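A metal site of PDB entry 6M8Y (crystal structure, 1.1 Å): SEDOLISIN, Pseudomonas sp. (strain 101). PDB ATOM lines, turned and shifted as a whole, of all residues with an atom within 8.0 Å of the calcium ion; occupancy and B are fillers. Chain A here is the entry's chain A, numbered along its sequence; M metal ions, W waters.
Five residues have an atom within 4 Å of the calcium ion: Asp 327, Val 328, Gly 343, Gly 345 and Asp 347. The nearest printed residue that does not touch the calcium ion is Thr 344 (4.1 Å).
OD2 of Asp 347 is bound to the calcium ion. The backbone carbonyl oxygen (O) of Gly 343 binds the calcium ion. OD1 of Asp 327 is bound to the calcium ion (2.3 Å). O of Gly 345 binds the calcium ion (2.3 Å). The calcium ion is bound by O of Val 328 (2.3 Å). Water W1 binds the calcium ion (2.4 Å).
Water W1 lies within hydrogen-bond range of the backbone carbonyl oxygen of Gly 351, the side-chain hydroxyl of Thr 350, the backbone NH of Val 328 and the backbone NH of Gly 353.
OD1 of Asp 347 sits at hydrogen-bond distance from OG1 of Thr 350, 2.7 Å away.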
ATOM      1  N   VAL A 218     -22.970  11.418  -2.082  1.00  0.00           N
ATOM      2  CA  VAL A 218     -22.134  10.512  -2.883  1.00  0.00           C
ATOM      3  C   VAL A 218     -20.673  10.768  -2.603  1.00  0.00           C
ATOM      4  O   VAL A 218     -20.244  11.929  -2.458  1.00  0.00           O
ATOM      5  CB  VAL A 218     -22.449  10.735  -4.371  1.00  0.00           C
ATOM      6  CG1 VAL A 218     -21.521   9.913  -5.278  1.00  0.00           C
ATOM      7  CG2 VAL A 218     -23.889  10.439  -4.697  1.00  0.00           C
ATOM      8  N   VAL A 325     -32.930   2.516   5.813  1.00  0.00           N
ATOM      9  CA  VAL A 325     -31.697   3.069   5.212  1.00  0.00           C
ATOM     10  C   VAL A 325     -31.623   4.574   5.396  1.00  0.00           C
ATOM     11  O   VAL A 325     -32.621   5.264   5.573  1.00  0.00           O
ATOM     12  CB  VAL A 325     -31.553   2.718   3.727  1.00  0.00           C
ATOM     13  CG1 VAL A 325     -31.368   1.226   3.534  1.00  0.00           C
ATOM     14  CG2 VAL A 325     -32.751   3.249   2.896  1.00  0.00           C
ATOM     15  N   HIS A 326     -30.421   5.082   5.244  1.00  0.00           N
ATOM     16  CA  HIS A 326     -30.148   6.484   4.978  1.00  0.00           C
ATOM     17  C   HIS A 326     -30.019   6.628   3.472  1.00  0.00           C
ATOM     18  O   HIS A 326     -29.058   6.190   2.872  1.00  0.00           O
ATOM     19  CB  HIS A 326     -28.874   6.955   5.628  1.00  0.00           C
ATOM     20  CG  HIS A 326     -28.826   6.841   7.082  1.00  0.00           C
ATOM     21  ND1 HIS A 326     -29.596   7.630   7.889  1.00  0.00           N
ATOM     22  CD2 HIS A 326     -28.098   6.092   7.905  1.00  0.00           C
ATOM     23  CE1 HIS A 326     -29.347   7.361   9.156  1.00  0.00           C
ATOM     24  NE2 HIS A 326     -28.466   6.411   9.230  1.00  0.00           N
ATOM     25  N   ASP A 327     -31.062   7.225   2.871  1.00  0.00           N
ATOM     26  CA  ASP A 327     -31.152   7.372   1.421  1.00  0.00           C
ATOM     27  C   ASP A 327     -30.252   8.512   0.970  1.00  0.00           C
ATOM     28  O   ASP A 327     -30.536   9.657   1.282  1.00  0.00           O
ATOM     29  CB  ASP A 327     -32.602   7.644   1.017  1.00  0.00           C
ATOM     30  CG  ASP A 327     -32.803   7.759  -0.475  1.00  0.00           C
ATOM     31  OD1 ASP A 327     -31.927   7.308  -1.243  1.00  0.00           O
ATOM     32  OD2 ASP A 327     -33.875   8.294  -0.868  1.00  0.00           O
ATOM     33  N   VAL A 328     -29.205   8.256   0.201  1.00  0.00           N
ATOM     34  CA  VAL A 328     -28.333   9.294  -0.315  1.00  0.00           C
ATOM     35  C   VAL A 328     -29.068   9.941  -1.495  1.00  0.00           C
ATOM     36  O   VAL A 328     -29.558   9.247  -2.376  1.00  0.00           O
ATOM     37  CB  VAL A 328     -26.976   8.701  -0.722  1.00  0.00           C
ATOM     38  CG1 VAL A 328     -26.131   9.775  -1.384  1.00  0.00           C
ATOM     39  CG2 VAL A 328     -26.282   8.098   0.482  1.00  0.00           C
ATOM     40  N   LYS A 329     -29.113  11.264  -1.506  1.00  0.00           N
ATOM     41  CA  LYS A 329     -29.837  12.011  -2.521  1.00  0.00           C
ATOM     42  C   LYS A 329     -29.003  12.988  -3.335  1.00  0.00           C
ATOM     43  O   LYS A 329     -29.454  13.428  -4.405  1.00  0.00           O
ATOM     44  CB  LYS A 329     -31.031  12.719  -1.898  1.00  0.00           C
ATOM     45  CG  LYS A 329     -32.079  11.763  -1.395  1.00  0.00           C
ATOM     46  CD  LYS A 329     -33.172  12.556  -0.650  1.00  0.00           C
ATOM     47  CE  LYS A 329     -34.304  11.702  -0.150  1.00  0.00           C
ATOM     48  NZ  LYS A 329     -35.615  12.428   0.039  1.00  0.00           N
ATOM     49  N   SER A 330     -27.812  13.373  -2.871  1.00  0.00           N
ATOM     50  CA  SER A 330     -27.024  14.430  -3.480  1.00  0.00           C
ATOM     51  C   SER A 330     -25.665  13.911  -3.982  1.00  0.00           C
ATOM     52  O   SER A 330     -24.973  13.247  -3.205  1.00  0.00           O
ATOM     53  CB  SER A 330     -26.752  15.557  -2.477  1.00  0.00           C
ATOM     54  OG  SER A 330     -25.833  16.511  -2.933  1.00  0.00           O
ATOM     55  N   ASN A 341     -26.285  10.322 -11.221  1.00  0.00           N
ATOM     56  CA  ASN A 341     -26.666  11.173 -10.091  1.00  0.00           C
ATOM     57  C   ASN A 341     -27.421  10.404  -9.021  1.00  0.00           C
ATOM     58  O   ASN A 341     -28.232   9.539  -9.314  1.00  0.00           O
ATOM     59  CB  ASN A 341     -27.601  12.300 -10.607  1.00  0.00           C
ATOM     60  CG  ASN A 341     -26.908  13.115 -11.673  1.00  0.00           C
ATOM     61  OD1 ASN A 341     -25.876  13.701 -11.423  1.00  0.00           O
ATOM     62  ND2 ASN A 341     -27.455  13.149 -12.874  1.00  0.00           N
ATOM     63  N   ALA A 342     -27.162  10.749  -7.761  1.00  0.00           N
ATOM     64  CA  ALA A 342     -27.988  10.213  -6.683  1.00  0.00           C
ATOM     65  C   ALA A 342     -29.403  10.788  -6.793  1.00  0.00           C
ATOM     66  O   ALA A 342     -29.627  11.837  -7.434  1.00  0.00           O
ATOM     67  CB  ALA A 342     -27.403  10.531  -5.315  1.00  0.00           C
ATOM     68  N   GLY A 343     -30.339  10.134  -6.153  1.00  0.00           N
ATOM     69  CA  GLY A 343     -31.693  10.575  -6.154  1.00  0.00           C
ATOM     70  C   GLY A 343     -32.501   9.819  -5.134  1.00  0.00           C
ATOM     71  O   GLY A 343     -31.953   9.037  -4.323  1.00  0.00           O
ATOM     72  N   THR A 344     -33.824  10.034  -5.136  1.00  0.00           N
ATOM     73  CA  THR A 344     -34.690   9.371  -4.205  1.00  0.00           C
ATOM     74  C   THR A 344     -34.675   7.873  -4.427  1.00  0.00           C
ATOM     75  O   THR A 344     -34.784   7.394  -5.575  1.00  0.00           O
ATOM     76  CB  THR A 344     -36.145   9.903  -4.407  1.00  0.00           C
ATOM     77  OG1 THR A 344     -36.101  11.288  -4.087  1.00  0.00           O
ATOM     78  CG2 THR A 344     -37.120   9.177  -3.529  1.00  0.00           C
ATOM     79  N   GLY A 345     -34.500   7.110  -3.372  1.00  0.00           N
ATOM     80  CA  GLY A 345     -34.483   5.672  -3.459  1.00  0.00           C
ATOM     81  C   GLY A 345     -33.206   5.128  -4.063  1.00  0.00           C
ATOM     82  O   GLY A 345     -32.111   5.746  -3.983  1.00  0.00           O
ATOM     83  N   TRP A 346     -33.271   3.949  -4.666  1.00  0.00           N
ATOM     84  CA  TRP A 346     -32.088   3.300  -5.218  1.00  0.00           C
ATOM     85  C   TRP A 346     -31.499   4.161  -6.330  1.00  0.00           C
ATOM     86  O   TRP A 346     -32.244   4.618  -7.201  1.00  0.00           O
ATOM     87  CB  TRP A 346     -32.461   1.913  -5.757  1.00  0.00           C
ATOM     88  CG  TRP A 346     -31.240   1.082  -6.072  1.00  0.00           C
ATOM     89  CD1 TRP A 346     -30.692   0.092  -5.270  1.00  0.00           C
ATOM     90  CD2 TRP A 346     -30.402   1.123  -7.230  1.00  0.00           C
ATOM     91  NE1 TRP A 346     -29.624  -0.468  -5.858  1.00  0.00           N
ATOM     92  CE2 TRP A 346     -29.388   0.155  -7.065  1.00  0.00           C
ATOM     93  CE3 TRP A 346     -30.392   1.871  -8.424  1.00  0.00           C
ATOM     94  CZ2 TRP A 346     -28.391  -0.034  -8.020  1.00  0.00           C
ATOM     95  CZ3 TRP A 346     -29.415   1.683  -9.364  1.00  0.00           C
ATOM     96  CH2 TRP A 346     -28.418   0.724  -9.128  1.00  0.00           C
ATOM     97  N   ASP A 347     -30.187   4.381  -6.334  1.00  0.00           N
ATOM     98  CA  ASP A 347     -29.520   5.091  -7.429  1.00  0.00           C
ATOM     99  C   ASP A 347     -28.207   4.403  -7.780  1.00  0.00           C
ATOM    100  O   ASP A 347     -27.678   3.571  -7.019  1.00  0.00           O
ATOM    101  CB  ASP A 347     -29.390   6.574  -7.102  1.00  0.00           C
ATOM    102  CG  ASP A 347     -28.635   6.856  -5.813  1.00  0.00           C
ATOM    103  OD1 ASP A 347     -27.495   6.383  -5.680  1.00  0.00           O
ATOM    104  OD2 ASP A 347     -29.250   7.565  -4.965  1.00  0.00           O
ATOM    105  N   TYR A 348     -27.655   4.742  -8.939  1.00  0.00           N
ATOM    106  CA  TYR A 348     -26.447   4.085  -9.397  1.00  0.00           C
ATOM    107  C   TYR A 348     -25.202   4.441  -8.568  1.00  0.00           C
ATOM    108  O   TYR A 348     -24.343   3.571  -8.418  1.00  0.00           O
ATOM    109  CB  TYR A 348     -26.223   4.340 -10.863  1.00  0.00           C
ATOM    110  CG  TYR A 348     -27.161   3.597 -11.774  1.00  0.00           C
ATOM    111  CD1 TYR A 348     -28.189   4.232 -12.473  1.00  0.00           C
ATOM    112  CD2 TYR A 348     -27.030   2.220 -11.937  1.00  0.00           C
ATOM    113  CE1 TYR A 348     -29.026   3.506 -13.289  1.00  0.00           C
ATOM    114  CE2 TYR A 348     -27.857   1.493 -12.767  1.00  0.00           C
ATOM    115  CZ  TYR A 348     -28.854   2.133 -13.439  1.00  0.00           C
ATOM    116  OH  TYR A 348     -29.669   1.370 -14.273  1.00  0.00           O
ATOM    117  N   PRO A 349     -25.021   5.653  -8.036  1.00  0.00           N
ATOM    118  CA  PRO A 349     -23.821   5.884  -7.225  1.00  0.00           C
ATOM    119  C   PRO A 349     -23.764   5.074  -5.918  1.00  0.00           C
ATOM    120  O   PRO A 349     -22.696   4.658  -5.483  1.00  0.00           O
ATOM    121  CB  PRO A 349     -23.805   7.391  -6.998  1.00  0.00           C
ATOM    122  CG  PRO A 349     -24.527   7.934  -8.208  1.00  0.00           C
ATOM    123  CD  PRO A 349     -25.658   6.944  -8.396  1.00  0.00           C
ATOM    124  N   THR A 350     -24.946   4.927  -5.285  1.00  0.00           N
ATOM    125  CA  THR A 350     -24.975   4.477  -3.922  1.00  0.00           C
ATOM    126  C   THR A 350     -25.921   3.343  -3.627  1.00  0.00           C
ATOM    127  O   THR A 350     -25.995   2.866  -2.458  1.00  0.00           O
ATOM    128  CB  THR A 350     -25.264   5.630  -2.920  1.00  0.00           C
ATOM    129  OG1 THR A 350     -26.533   6.212  -3.148  1.00  0.00           O
ATOM    130  CG2 THR A 350     -24.166   6.678  -3.001  1.00  0.00           C
ATOM    131  N   GLY A 351     -26.674   2.853  -4.597  1.00  0.00           N
ATOM    132  CA  GLY A 351     -27.656   1.826  -4.343  1.00  0.00           C
ATOM    133  C   GLY A 351     -28.718   2.318  -3.390  1.00  0.00           C
ATOM    134  O   GLY A 351     -29.229   3.450  -3.541  1.00  0.00           O
ATOM    135  N   TRP A 352     -29.073   1.528  -2.379  1.00  0.00           N
ATOM    136  CA  TRP A 352     -30.080   1.955  -1.405  1.00  0.00           C
ATOM    137  C   TRP A 352     -29.530   2.948  -0.386  1.00  0.00           C
ATOM    138  O   TRP A 352     -30.327   3.449   0.415  1.00  0.00           O
ATOM    139  CB  TRP A 352     -30.615   0.720  -0.674  1.00  0.00           C
ATOM    140  CG  TRP A 352     -31.442  -0.192  -1.495  1.00  0.00           C
ATOM    141  CD1 TRP A 352     -31.162  -1.470  -1.847  1.00  0.00           C
ATOM    142  CD2 TRP A 352     -32.719   0.104  -2.058  1.00  0.00           C
ATOM    143  NE1 TRP A 352     -32.165  -2.009  -2.582  1.00  0.00           N
ATOM    144  CE2 TRP A 352     -33.150  -1.040  -2.747  1.00  0.00           C
ATOM    145  CE3 TRP A 352     -33.576   1.235  -2.070  1.00  0.00           C
ATOM    146  CZ2 TRP A 352     -34.373  -1.114  -3.436  1.00  0.00           C
ATOM    147  CZ3 TRP A 352     -34.738   1.154  -2.731  1.00  0.00           C
ATOM    148  CH2 TRP A 352     -35.158  -0.004  -3.418  1.00  0.00           C
ATOM    149  N   GLY A 353     -28.249   3.199  -0.350  1.00  0.00           N
ATOM    150  CA  GLY A 353     -27.627   3.994   0.713  1.00  0.00           C
ATOM    151  C   GLY A 353     -27.124   3.129   1.843  1.00  0.00           C
ATOM    152  O   GLY A 353     -26.843   1.940   1.637  1.00  0.00           O
HETATM  153 CA    CA M   1     -30.732   7.430  -3.213  1.00  0.00          CA
HETATM  154  O   HOH W   1     -29.159   5.891  -2.215  1.00  0.00           O
